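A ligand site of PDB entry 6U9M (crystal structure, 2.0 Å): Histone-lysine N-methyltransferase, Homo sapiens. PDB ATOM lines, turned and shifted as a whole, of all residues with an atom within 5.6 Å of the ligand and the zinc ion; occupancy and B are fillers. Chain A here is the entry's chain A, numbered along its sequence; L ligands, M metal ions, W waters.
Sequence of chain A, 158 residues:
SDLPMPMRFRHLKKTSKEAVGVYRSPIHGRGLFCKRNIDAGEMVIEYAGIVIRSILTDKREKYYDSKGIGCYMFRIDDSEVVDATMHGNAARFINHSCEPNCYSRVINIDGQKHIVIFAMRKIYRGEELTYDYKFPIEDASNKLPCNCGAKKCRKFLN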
ATOM      1  N   ILE A  27      26.537 -20.624  -4.418  1.00  0.00           N
ATOM      2  CA  ILE A  27      26.583 -22.017  -4.888  1.00  0.00           C
ATOM      3  C   ILE A  27      25.369 -22.212  -5.793  1.00  0.00           C
ATOM      4  O   ILE A  27      25.540 -22.549  -6.963  1.00  0.00           O
ATOM      5  CB  ILE A  27      26.665 -23.050  -3.714  1.00  0.00           C
ATOM      6  CG1 ILE A  27      28.012 -22.926  -2.955  1.00  0.00           C
ATOM      7  CG2 ILE A  27      26.497 -24.469  -4.235  1.00  0.00           C
ATOM      8  CD1 ILE A  27      27.999 -23.594  -1.479  1.00  0.00           C
ATOM      9  N   HIS A  28      24.155 -21.990  -5.257  1.00  0.00           N
ATOM     10  CA  HIS A  28      22.885 -22.089  -6.002  1.00  0.00           C
ATOM     11  C   HIS A  28      21.746 -21.446  -5.220  1.00  0.00           C
ATOM     12  O   HIS A  28      21.582 -21.747  -4.032  1.00  0.00           O
ATOM     13  CB  HIS A  28      22.546 -23.558  -6.306  1.00  0.00           C
ATOM     14  CG  HIS A  28      21.291 -23.756  -7.091  1.00  0.00           C
ATOM     15  ND1 HIS A  28      20.028 -23.676  -6.492  1.00  0.00           N
ATOM     16  CD2 HIS A  28      21.133 -24.087  -8.398  1.00  0.00           C
ATOM     17  CE1 HIS A  28      19.166 -23.930  -7.454  1.00  0.00           C
ATOM     18  NE2 HIS A  28      19.780 -24.228  -8.611  1.00  0.00           N
ATOM     19  N   GLY A  29      20.918 -20.659  -5.927  1.00  0.00           N
ATOM     20  CA  GLY A  29      19.692 -20.032  -5.403  1.00  0.00           C
ATOM     21  C   GLY A  29      19.760 -19.521  -3.983  1.00  0.00           C
ATOM     22  O   GLY A  29      20.469 -18.555  -3.700  1.00  0.00           O
ATOM     23  N   ARG A  30      19.038 -20.177  -3.066  1.00  0.00           N
ATOM     24  CA  ARG A  30      19.108 -19.815  -1.641  1.00  0.00           C
ATOM     25  C   ARG A  30      19.848 -20.920  -0.892  1.00  0.00           C
ATOM     26  O   ARG A  30      19.799 -22.091  -1.306  1.00  0.00           O
ATOM     27  CB  ARG A  30      17.711 -19.541  -1.010  1.00  0.00           C
ATOM     28  CG  ARG A  30      17.108 -18.179  -1.412  1.00  0.00           C
ATOM     29  CD  ARG A  30      15.698 -17.990  -0.888  1.00  0.00           C
ATOM     30  NE  ARG A  30      14.768 -18.918  -1.538  1.00  0.00           N
ATOM     31  CZ  ARG A  30      13.505 -19.128  -1.172  1.00  0.00           C
ATOM     32  NH1 ARG A  30      13.002 -18.490  -0.113  1.00  0.00           N
ATOM     33  NH2 ARG A  30      12.742 -19.987  -1.829  1.00  0.00           N
ATOM     34  N   GLY A  31      20.523 -20.555   0.179  1.00  0.00           N
ATOM     35  CA  GLY A  31      21.230 -21.513   1.015  1.00  0.00           C
ATOM     36  C   GLY A  31      20.973 -21.263   2.481  1.00  0.00           C
ATOM     37  O   GLY A  31      20.340 -20.254   2.844  1.00  0.00           O
ATOM     38  N   GLY A  70       8.097 -25.506  -5.860  1.00  0.00           N
ATOM     39  CA  GLY A  70       9.408 -26.122  -5.746  1.00  0.00           C
ATOM     40  C   GLY A  70       9.317 -27.405  -4.932  1.00  0.00           C
ATOM     41  O   GLY A  70       8.650 -27.432  -3.905  1.00  0.00           O
ATOM     42  N   CYS A  71       9.926 -28.492  -5.428  1.00  0.00           N
ATOM     43  CA  CYS A  71       9.889 -29.812  -4.795  1.00  0.00           C
ATOM     44  C   CYS A  71      11.146 -30.007  -3.960  1.00  0.00           C
ATOM     45  O   CYS A  71      12.234 -29.962  -4.507  1.00  0.00           O
ATOM     46  CB  CYS A  71       9.752 -30.910  -5.853  1.00  0.00           C
ATOM     47  SG  CYS A  71       9.786 -32.587  -5.162  1.00  0.00           S
ATOM     48  N   TYR A  72      11.008 -30.220  -2.640  1.00  0.00           N
ATOM     49  CA  TYR A  72      12.136 -30.356  -1.708  1.00  0.00           C
ATOM     50  C   TYR A  72      12.072 -31.737  -1.095  1.00  0.00           C
ATOM     51  O   TYR A  72      11.197 -31.991  -0.282  1.00  0.00           O
ATOM     52  CB  TYR A  72      12.073 -29.266  -0.605  1.00  0.00           C
ATOM     53  CG  TYR A  72      12.357 -27.872  -1.129  1.00  0.00           C
ATOM     54  CD1 TYR A  72      13.640 -27.336  -1.082  1.00  0.00           C
ATOM     55  CD2 TYR A  72      11.355 -27.103  -1.716  1.00  0.00           C
ATOM     56  CE1 TYR A  72      13.913 -26.061  -1.582  1.00  0.00           C
ATOM     57  CE2 TYR A  72      11.624 -25.832  -2.237  1.00  0.00           C
ATOM     58  CZ  TYR A  72      12.911 -25.329  -2.190  1.00  0.00           C
ATOM     59  OH  TYR A  72      13.210 -24.094  -2.692  1.00  0.00           O
ATOM     60  N   ARG A  92      15.746 -27.411   4.301  1.00  0.00           N
ATOM     61  CA  ARG A  92      15.503 -27.793   2.901  1.00  0.00           C
ATOM     62  C   ARG A  92      16.333 -26.978   1.887  1.00  0.00           C
ATOM     63  O   ARG A  92      16.461 -27.383   0.738  1.00  0.00           O
ATOM     64  CB  ARG A  92      13.987 -27.781   2.561  1.00  0.00           C
ATOM     65  CG  ARG A  92      13.376 -26.416   2.341  1.00  0.00           C
ATOM     66  CD  ARG A  92      11.848 -26.552   2.392  1.00  0.00           C
ATOM     67  NE  ARG A  92      11.183 -25.306   2.009  1.00  0.00           N
ATOM     68  CZ  ARG A  92      10.828 -24.346   2.855  1.00  0.00           C
ATOM     69  NH1 ARG A  92      11.080 -24.468   4.157  1.00  0.00           N
ATOM     70  NH2 ARG A  92      10.218 -23.259   2.407  1.00  0.00           N
ATOM     71  N   PHE A  93      16.927 -25.837   2.321  1.00  0.00           N
ATOM     72  CA  PHE A  93      17.760 -24.993   1.473  1.00  0.00           C
ATOM     73  C   PHE A  93      19.272 -25.374   1.515  1.00  0.00           C
ATOM     74  O   PHE A  93      20.040 -24.773   0.780  1.00  0.00           O
ATOM     75  CB  PHE A  93      17.553 -23.514   1.806  1.00  0.00           C
ATOM     76  CG  PHE A  93      16.135 -23.041   1.544  1.00  0.00           C
ATOM     77  CD1 PHE A  93      15.695 -22.780   0.243  1.00  0.00           C
ATOM     78  CD2 PHE A  93      15.208 -22.963   2.574  1.00  0.00           C
ATOM     79  CE1 PHE A  93      14.382 -22.385   0.003  1.00  0.00           C
ATOM     80  CE2 PHE A  93      13.901 -22.537   2.336  1.00  0.00           C
ATOM     81  CZ  PHE A  93      13.491 -22.260   1.050  1.00  0.00           C
ATOM     82  N   ILE A  94      19.675 -26.354   2.349  1.00  0.00           N
ATOM     83  CA  ILE A  94      21.095 -26.769   2.452  1.00  0.00           C
ATOM     84  C   ILE A  94      21.619 -27.270   1.096  1.00  0.00           C
ATOM     85  O   ILE A  94      21.095 -28.243   0.552  1.00  0.00           O
ATOM     86  CB  ILE A  94      21.414 -27.764   3.614  1.00  0.00           C
ATOM     87  CG1 ILE A  94      20.905 -27.246   4.969  1.00  0.00           C
ATOM     88  CG2 ILE A  94      22.948 -28.077   3.695  1.00  0.00           C
ATOM     89  CD1 ILE A  94      20.800 -28.273   6.034  1.00  0.00           C
ATOM     90  N   ASN A  95      22.603 -26.569   0.541  1.00  0.00           N
ATOM     91  CA  ASN A  95      23.239 -26.912  -0.736  1.00  0.00           C
ATOM     92  C   ASN A  95      24.300 -27.976  -0.560  1.00  0.00           C
ATOM     93  O   ASN A  95      24.712 -28.238   0.570  1.00  0.00           O
ATOM     94  CB  ASN A  95      23.869 -25.654  -1.381  1.00  0.00           C
ATOM     95  CG  ASN A  95      22.810 -24.775  -2.018  1.00  0.00           C
ATOM     96  OD1 ASN A  95      21.840 -25.263  -2.612  1.00  0.00           O
ATOM     97  ND2 ASN A  95      22.962 -23.466  -1.890  1.00  0.00           N
ATOM     98  N   HIS A  96      24.737 -28.595  -1.665  1.00  0.00           N
ATOM     99  CA  HIS A  96      25.810 -29.614  -1.685  1.00  0.00           C
ATOM    100  C   HIS A  96      27.198 -28.954  -1.713  1.00  0.00           C
ATOM    101  O   HIS A  96      27.347 -27.894  -2.321  1.00  0.00           O
ATOM    102  CB  HIS A  96      25.689 -30.498  -2.948  1.00  0.00           C
ATOM    103  CG  HIS A  96      26.878 -31.380  -3.196  1.00  0.00           C
ATOM    104  ND1 HIS A  96      27.033 -32.572  -2.516  1.00  0.00           N
ATOM    105  CD2 HIS A  96      27.966 -31.175  -3.966  1.00  0.00           C
ATOM    106  CE1 HIS A  96      28.180 -33.075  -2.927  1.00  0.00           C
ATOM    107  NE2 HIS A  96      28.787 -32.269  -3.794  1.00  0.00           N
ATOM    108  N   SER A  97      28.221 -29.623  -1.130  1.00  0.00           N
ATOM    109  CA  SER A  97      29.658 -29.260  -1.225  1.00  0.00           C
ATOM    110  C   SER A  97      30.511 -30.488  -1.131  1.00  0.00           C
ATOM    111  O   SER A  97      30.233 -31.368  -0.323  1.00  0.00           O
ATOM    112  CB  SER A  97      30.093 -28.247  -0.176  1.00  0.00           C
ATOM    113  OG  SER A  97      31.467 -27.910  -0.323  1.00  0.00           O
ATOM    114  N   CYS A  98      31.611 -30.525  -1.920  1.00  0.00           N
ATOM    115  CA  CYS A  98      32.587 -31.611  -1.979  1.00  0.00           C
ATOM    116  C   CYS A  98      33.540 -31.554  -0.798  1.00  0.00           C
ATOM    117  O   CYS A  98      34.278 -32.516  -0.528  1.00  0.00           O
ATOM    118  CB  CYS A  98      33.315 -31.601  -3.320  1.00  0.00           C
ATOM    119  SG  CYS A  98      32.200 -31.636  -4.736  1.00  0.00           S
ATOM    120  N   TYR A 133      25.837 -34.462  -0.896  1.00  0.00           N
ATOM    121  CA  TYR A 133      24.649 -35.142  -1.435  1.00  0.00           C
ATOM    122  C   TYR A 133      25.191 -36.473  -2.003  1.00  0.00           C
ATOM    123  O   TYR A 133      26.246 -36.467  -2.666  1.00  0.00           O
ATOM    124  CB  TYR A 133      24.026 -34.366  -2.623  1.00  0.00           C
ATOM    125  CG  TYR A 133      23.253 -33.085  -2.353  1.00  0.00           C
ATOM    126  CD1 TYR A 133      23.339 -32.433  -1.125  1.00  0.00           C
ATOM    127  CD2 TYR A 133      22.507 -32.484  -3.347  1.00  0.00           C
ATOM    128  CE1 TYR A 133      22.660 -31.229  -0.891  1.00  0.00           C
ATOM    129  CE2 TYR A 133      21.847 -31.281  -3.140  1.00  0.00           C
ATOM    130  CZ  TYR A 133      21.914 -30.665  -1.906  1.00  0.00           C
ATOM    131  OH  TYR A 133      21.244 -29.479  -1.740  1.00  0.00           O
ATOM    132  N   PRO A 145      26.306 -30.431 -12.822  1.00  0.00           N
ATOM    133  CA  PRO A 145      27.561 -29.728 -12.467  1.00  0.00           C
ATOM    134  C   PRO A 145      27.588 -29.095 -11.075  1.00  0.00           C
ATOM    135  O   PRO A 145      26.640 -28.428 -10.681  1.00  0.00           O
ATOM    136  CB  PRO A 145      27.729 -28.687 -13.584  1.00  0.00           C
ATOM    137  CG  PRO A 145      26.379 -28.498 -14.149  1.00  0.00           C
ATOM    138  CD  PRO A 145      25.631 -29.791 -13.971  1.00  0.00           C
ATOM    139  N   CYS A 146      28.692 -29.302 -10.333  1.00  0.00           N
ATOM    140  CA  CYS A 146      28.859 -28.781  -8.976  1.00  0.00           C
ATOM    141  C   CYS A 146      29.512 -27.407  -8.924  1.00  0.00           C
ATOM    142  O   CYS A 146      30.572 -27.178  -9.537  1.00  0.00           O
ATOM    143  CB  CYS A 146      29.595 -29.777  -8.088  1.00  0.00           C
ATOM    144  SG  CYS A 146      29.664 -29.279  -6.360  1.00  0.00           S
ATOM    145  N   ASN A 147      28.911 -26.516  -8.125  1.00  0.00           N
ATOM    146  CA  ASN A 147      29.339 -25.133  -7.943  1.00  0.00           C
ATOM    147  C   ASN A 147      29.851 -24.809  -6.514  1.00  0.00           C
ATOM    148  O   ASN A 147      29.939 -23.639  -6.154  1.00  0.00           O
ATOM    149  CB  ASN A 147      28.218 -24.184  -8.360  1.00  0.00           C
ATOM    150  CG  ASN A 147      28.684 -22.797  -8.700  1.00  0.00           C
ATOM    151  OD1 ASN A 147      29.578 -22.584  -9.528  1.00  0.00           O
ATOM    152  ND2 ASN A 147      28.071 -21.802  -8.057  1.00  0.00           N
ATOM    153  N   CYS A 148      30.238 -25.837  -5.724  1.00  0.00           N
ATOM    154  CA  CYS A 148      30.748 -25.593  -4.368  1.00  0.00           C
ATOM    155  C   CYS A 148      32.033 -24.747  -4.364  1.00  0.00           C
ATOM    156  O   CYS A 148      32.300 -24.045  -3.383  1.00  0.00           O
ATOM    157  CB  CYS A 148      30.936 -26.901  -3.599  1.00  0.00           C
ATOM    158  SG  CYS A 148      32.394 -27.860  -4.084  1.00  0.00           S
ATOM    159  N   GLY A 149      32.816 -24.871  -5.442  1.00  0.00           N
ATOM    160  CA  GLY A 149      34.057 -24.154  -5.670  1.00  0.00           C
ATOM    161  C   GLY A 149      35.270 -24.679  -4.928  1.00  0.00           C
ATOM    162  O   GLY A 149      36.335 -24.059  -5.012  1.00  0.00           O
ATOM    163  N   ALA A 150      35.149 -25.812  -4.192  1.00  0.00           N
ATOM    164  CA  ALA A 150      36.257 -26.403  -3.404  1.00  0.00           C
ATOM    165  C   ALA A 150      37.468 -26.802  -4.286  1.00  0.00           C
ATOM    166  O   ALA A 150      37.295 -27.099  -5.467  1.00  0.00           O
ATOM    167  CB  ALA A 150      35.767 -27.598  -2.599  1.00  0.00           C
ATOM    168  N   CYS A 153      36.992 -30.373  -5.570  1.00  0.00           N
ATOM    169  CA  CYS A 153      35.636 -30.523  -6.095  1.00  0.00           C
ATOM    170  C   CYS A 153      35.517 -31.744  -7.023  1.00  0.00           C
ATOM    171  O   CYS A 153      36.364 -31.929  -7.879  1.00  0.00           O
ATOM    172  CB  CYS A 153      35.177 -29.247  -6.778  1.00  0.00           C
ATOM    173  SG  CYS A 153      33.482 -29.310  -7.425  1.00  0.00           S
ATOM    174  N   ARG A 154      34.461 -32.564  -6.830  1.00  0.00           N
ATOM    175  CA  ARG A 154      34.139 -33.743  -7.644  1.00  0.00           C
ATOM    176  C   ARG A 154      33.563 -33.324  -9.021  1.00  0.00           C
ATOM    177  O   ARG A 154      33.405 -34.172  -9.904  1.00  0.00           O
ATOM    178  CB  ARG A 154      33.154 -34.665  -6.900  1.00  0.00           C
ATOM    179  N   LYS A 155      33.227 -32.019  -9.169  1.00  0.00           N
ATOM    180  CA  LYS A 155      32.732 -31.313 -10.365  1.00  0.00           C
ATOM    181  C   LYS A 155      31.298 -31.696 -10.795  1.00  0.00           C
ATOM    182  O   LYS A 155      30.727 -31.017 -11.656  1.00  0.00           O
ATOM    183  CB  LYS A 155      33.731 -31.433 -11.535  1.00  0.00           C
ATOM    184  CG  LYS A 155      35.144 -30.915 -11.186  1.00  0.00           C
ATOM    185  CD  LYS A 155      35.189 -29.395 -10.969  1.00  0.00           C
ATOM    186  CE  LYS A 155      36.592 -28.886 -10.718  1.00  0.00           C
ATOM    187  NZ  LYS A 155      36.639 -27.392 -10.743  1.00  0.00           N
ATOM    188  N   LEU A 157      27.339 -33.515  -8.946  1.00  0.00           N
ATOM    189  CA  LEU A 157      26.618 -33.931  -7.735  1.00  0.00           C
ATOM    190  C   LEU A 157      26.466 -35.461  -7.674  1.00  0.00           C
ATOM    191  O   LEU A 157      26.540 -36.045  -6.591  1.00  0.00           O
ATOM    192  CB  LEU A 157      25.235 -33.270  -7.613  1.00  0.00           C
ATOM    193  CG  LEU A 157      25.114 -31.736  -7.751  1.00  0.00           C
ATOM    194  CD1 LEU A 157      23.671 -31.325  -7.631  1.00  0.00           C
ATOM    195  CD2 LEU A 157      25.915 -30.998  -6.709  1.00  0.00           C
HETATM  196  C1  LIG L   1      25.167 -26.810  -8.163  1.00  0.00           C
HETATM  197  C2  LIG L   1      23.541 -27.177  -6.601  1.00  0.00           C
HETATM  198  C3  LIG L   1      24.525 -27.414  -5.590  1.00  0.00           C
HETATM  199  C4  LIG L   1      22.613 -27.590  -4.591  1.00  0.00           C
HETATM  200  C5  LIG L   1      20.993 -27.312  -6.584  1.00  0.00           C
HETATM  201  C6  LIG L   1      20.758 -28.647  -7.367  1.00  0.00           C
HETATM  202  C7  LIG L   1      20.088 -29.488  -6.268  1.00  0.00           C
HETATM  203  C8  LIG L   1      19.203 -28.407  -5.630  1.00  0.00           C
HETATM  204  O1  LIG L   1      19.334 -30.555  -6.760  1.00  0.00           O
HETATM  205  N1  LIG L   1      26.225 -27.038  -7.297  1.00  0.00           N
HETATM  206  N2  LIG L   1      23.827 -26.868  -7.921  1.00  0.00           N
HETATM  207  N3  LIG L   1      26.897 -27.615  -5.127  1.00  0.00           N
HETATM  208  C9  LIG L   1      25.902 -27.352  -5.997  1.00  0.00           C
HETATM  209  O2  LIG L   1      19.899 -28.314  -8.405  1.00  0.00           O
HETATM  210  O3  LIG L   1      15.924 -24.113  -3.254  1.00  0.00           O
HETATM  211  C10 LIG L   1      17.089 -23.762  -3.409  1.00  0.00           C
HETATM  212  O4  LIG L   1      17.353 -22.465  -3.648  1.00  0.00           O
HETATM  213  C11 LIG L   1      18.340 -24.682  -3.389  1.00  0.00           C
HETATM  214  N4  LIG L   1      19.608 -23.932  -3.360  1.00  0.00           N
HETATM  215  C12 LIG L   1      18.238 -25.583  -2.102  1.00  0.00           C
HETATM  216  C13 LIG L   1      18.727 -27.039  -2.364  1.00  0.00           C
HETATM  217  N5  LIG L   1      18.012 -27.669  -3.568  1.00  0.00           N
HETATM  218  C14 LIG L   1      16.545 -27.971  -3.382  1.00  0.00           C
HETATM  219  C15 LIG L   1      15.852 -28.025  -4.784  1.00  0.00           C
HETATM  220  C16 LIG L   1      14.315 -27.795  -4.905  1.00  0.00           C
HETATM  221  N6  LIG L   1      14.565 -26.815  -6.045  1.00  0.00           N
HETATM  222  C17 LIG L   1      13.778 -25.546  -6.024  1.00  0.00           C
HETATM  223  C18 LIG L   1      14.316 -24.611  -7.059  1.00  0.00           C
HETATM  224  S1  LIG L   1      14.812 -25.174  -8.620  1.00  0.00           S
HETATM  225  C19 LIG L   1      15.289 -23.601  -9.104  1.00  0.00           C
HETATM  226  C20 LIG L   1      15.087 -22.686  -8.136  1.00  0.00           C
HETATM  227  C21 LIG L   1      14.512 -23.263  -6.942  1.00  0.00           C
HETATM  228  C22 LIG L   1      16.006 -26.717  -5.642  1.00  0.00           C
HETATM  229  C23 LIG L   1      18.813 -28.805  -4.180  1.00  0.00           C
HETATM  230  O5  LIG L   1      19.972 -27.196  -5.635  1.00  0.00           O
HETATM  231  N7  LIG L   1      22.319 -27.312  -5.965  1.00  0.00           N
HETATM  232  N8  LIG L   1      23.913 -27.661  -4.348  1.00  0.00           N
HETATM  233 ZN    ZN M   1      31.921 -29.559  -5.513  1.00  0.00          ZN
HETATM  234  O   HOH W   1      15.321 -20.669  -3.771  1.00  0.00           O
HETATM  235  O   HOH W   2      14.936 -28.448  -8.399  1.00  0.00           O
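The backbone carbonyl oxygen of Ile 27 sits at hydrogen-bond distance from the side-chain amide nitrogen of Asn 147.
A ring nitrogen (ND1) of His 96 sits at hydrogen-bond distance from the backbone NH of Tyr 133, 2.8 Å away.
N of Cys 146 is in hydrogen-bond range of O of Lys 155, at 3.0 Å.
A ring nitrogen (NE2) of His 96 sits close to the side-chain sulfur of Cys 98, at 3.6 Å.
The side-chain hydroxyl (OH) of Tyr 133 lies within hydrogen-bond range of the backbone carbonyl oxygen (O) of Ile 94.
SG of Cys 153 lies close to N of Lys 155, at 3.2 Å.
The backbone NH (N) of Arg 154 sits close to the side-chain sulfur (SG) of Cys 98, at 3.2 Å.
The side-chain amide nitrogen (ND2) of Asn 95 is in hydrogen-bond range of the backbone carbonyl oxygen (O) of Arg 30 (3.5 Å).
Residues that only touch the ligand: Ile 27 (3.3 Å), Gly 29 (3.8 Å), Cys 71 (3.0 Å), Arg 92 (3.8 Å), Phe 93 (3.5 Å), Ile 94 (3.9 Å), Tyr 133 (3.5 Å), Pro 145 (3.3 Å) and Leu 157 (3.7 Å).
Hydrophobic or aromatic side chains that line the ligand: Ile 27, His 28, Tyr 72, Phe 93, His 96 and Leu 157.
The nearest printed residue that does not touch the ligand is Gly 70 (4.4 Å).
Four residues have an atom within 4 Å of the zinc ion: Cys 98, Cys 146, Cys 148 and Cys 153.
The zinc ion is bound by the side-chain sulfur of Cys 98 (2.2 Å), the side-chain sulfur of Cys 148 (2.3 Å), the side-chain sulfur of Cys 146 (2.4 Å) and the side-chain sulfur of Cys 153 (2.5 Å).
The zinc ion has four donor atoms within binding distance.
The backbone NH of His 96 lies within hydrogen-bond range of a nitrogen (N8) of the ligand, at 3.0 Å.
The side-chain sulfur (SG) of Cys 146 sits close to a nitrogen (N3) of the ligand (3.5 Å).
A ring nitrogen (ND1) of His 28 sits at hydrogen-bond distance from a nitrogen (N4) of the ligand.
A nitrogen (N4) of the ligand sits at hydrogen-bond distance from the side-chain amide oxygen (OD1) of Asn 95, 2.7 Å away.
N4 of the ligand is in hydrogen-bond range of O of His 28, at 3.0 Å.
The backbone NH (N) of Asn 147 is in hydrogen-bond range of a nitrogen (N1) of the ligand, 2.9 Å away.
A nitrogen (N4) of the ligand is in hydrogen-bond range of the backbone carbonyl oxygen of Arg 30, 2.8 Å away.
The side-chain hydroxyl of Tyr 72 sits at hydrogen-bond distance from an oxygen (O3) of the ligand, 2.8 Å away.
The backbone NH of Arg 30 is in hydrogen-bond range of an oxygen (O4) of the ligand, 2.9 Å away.
The backbone carbonyl oxygen (O) of His 96 is in hydrogen-bond range of a nitrogen (N3) of the ligand (2.9 Å).
Water W1 lies within hydrogen-bond range of an oxygen (O4) of the ligand and the guanidinium group (NE) of Arg 30.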
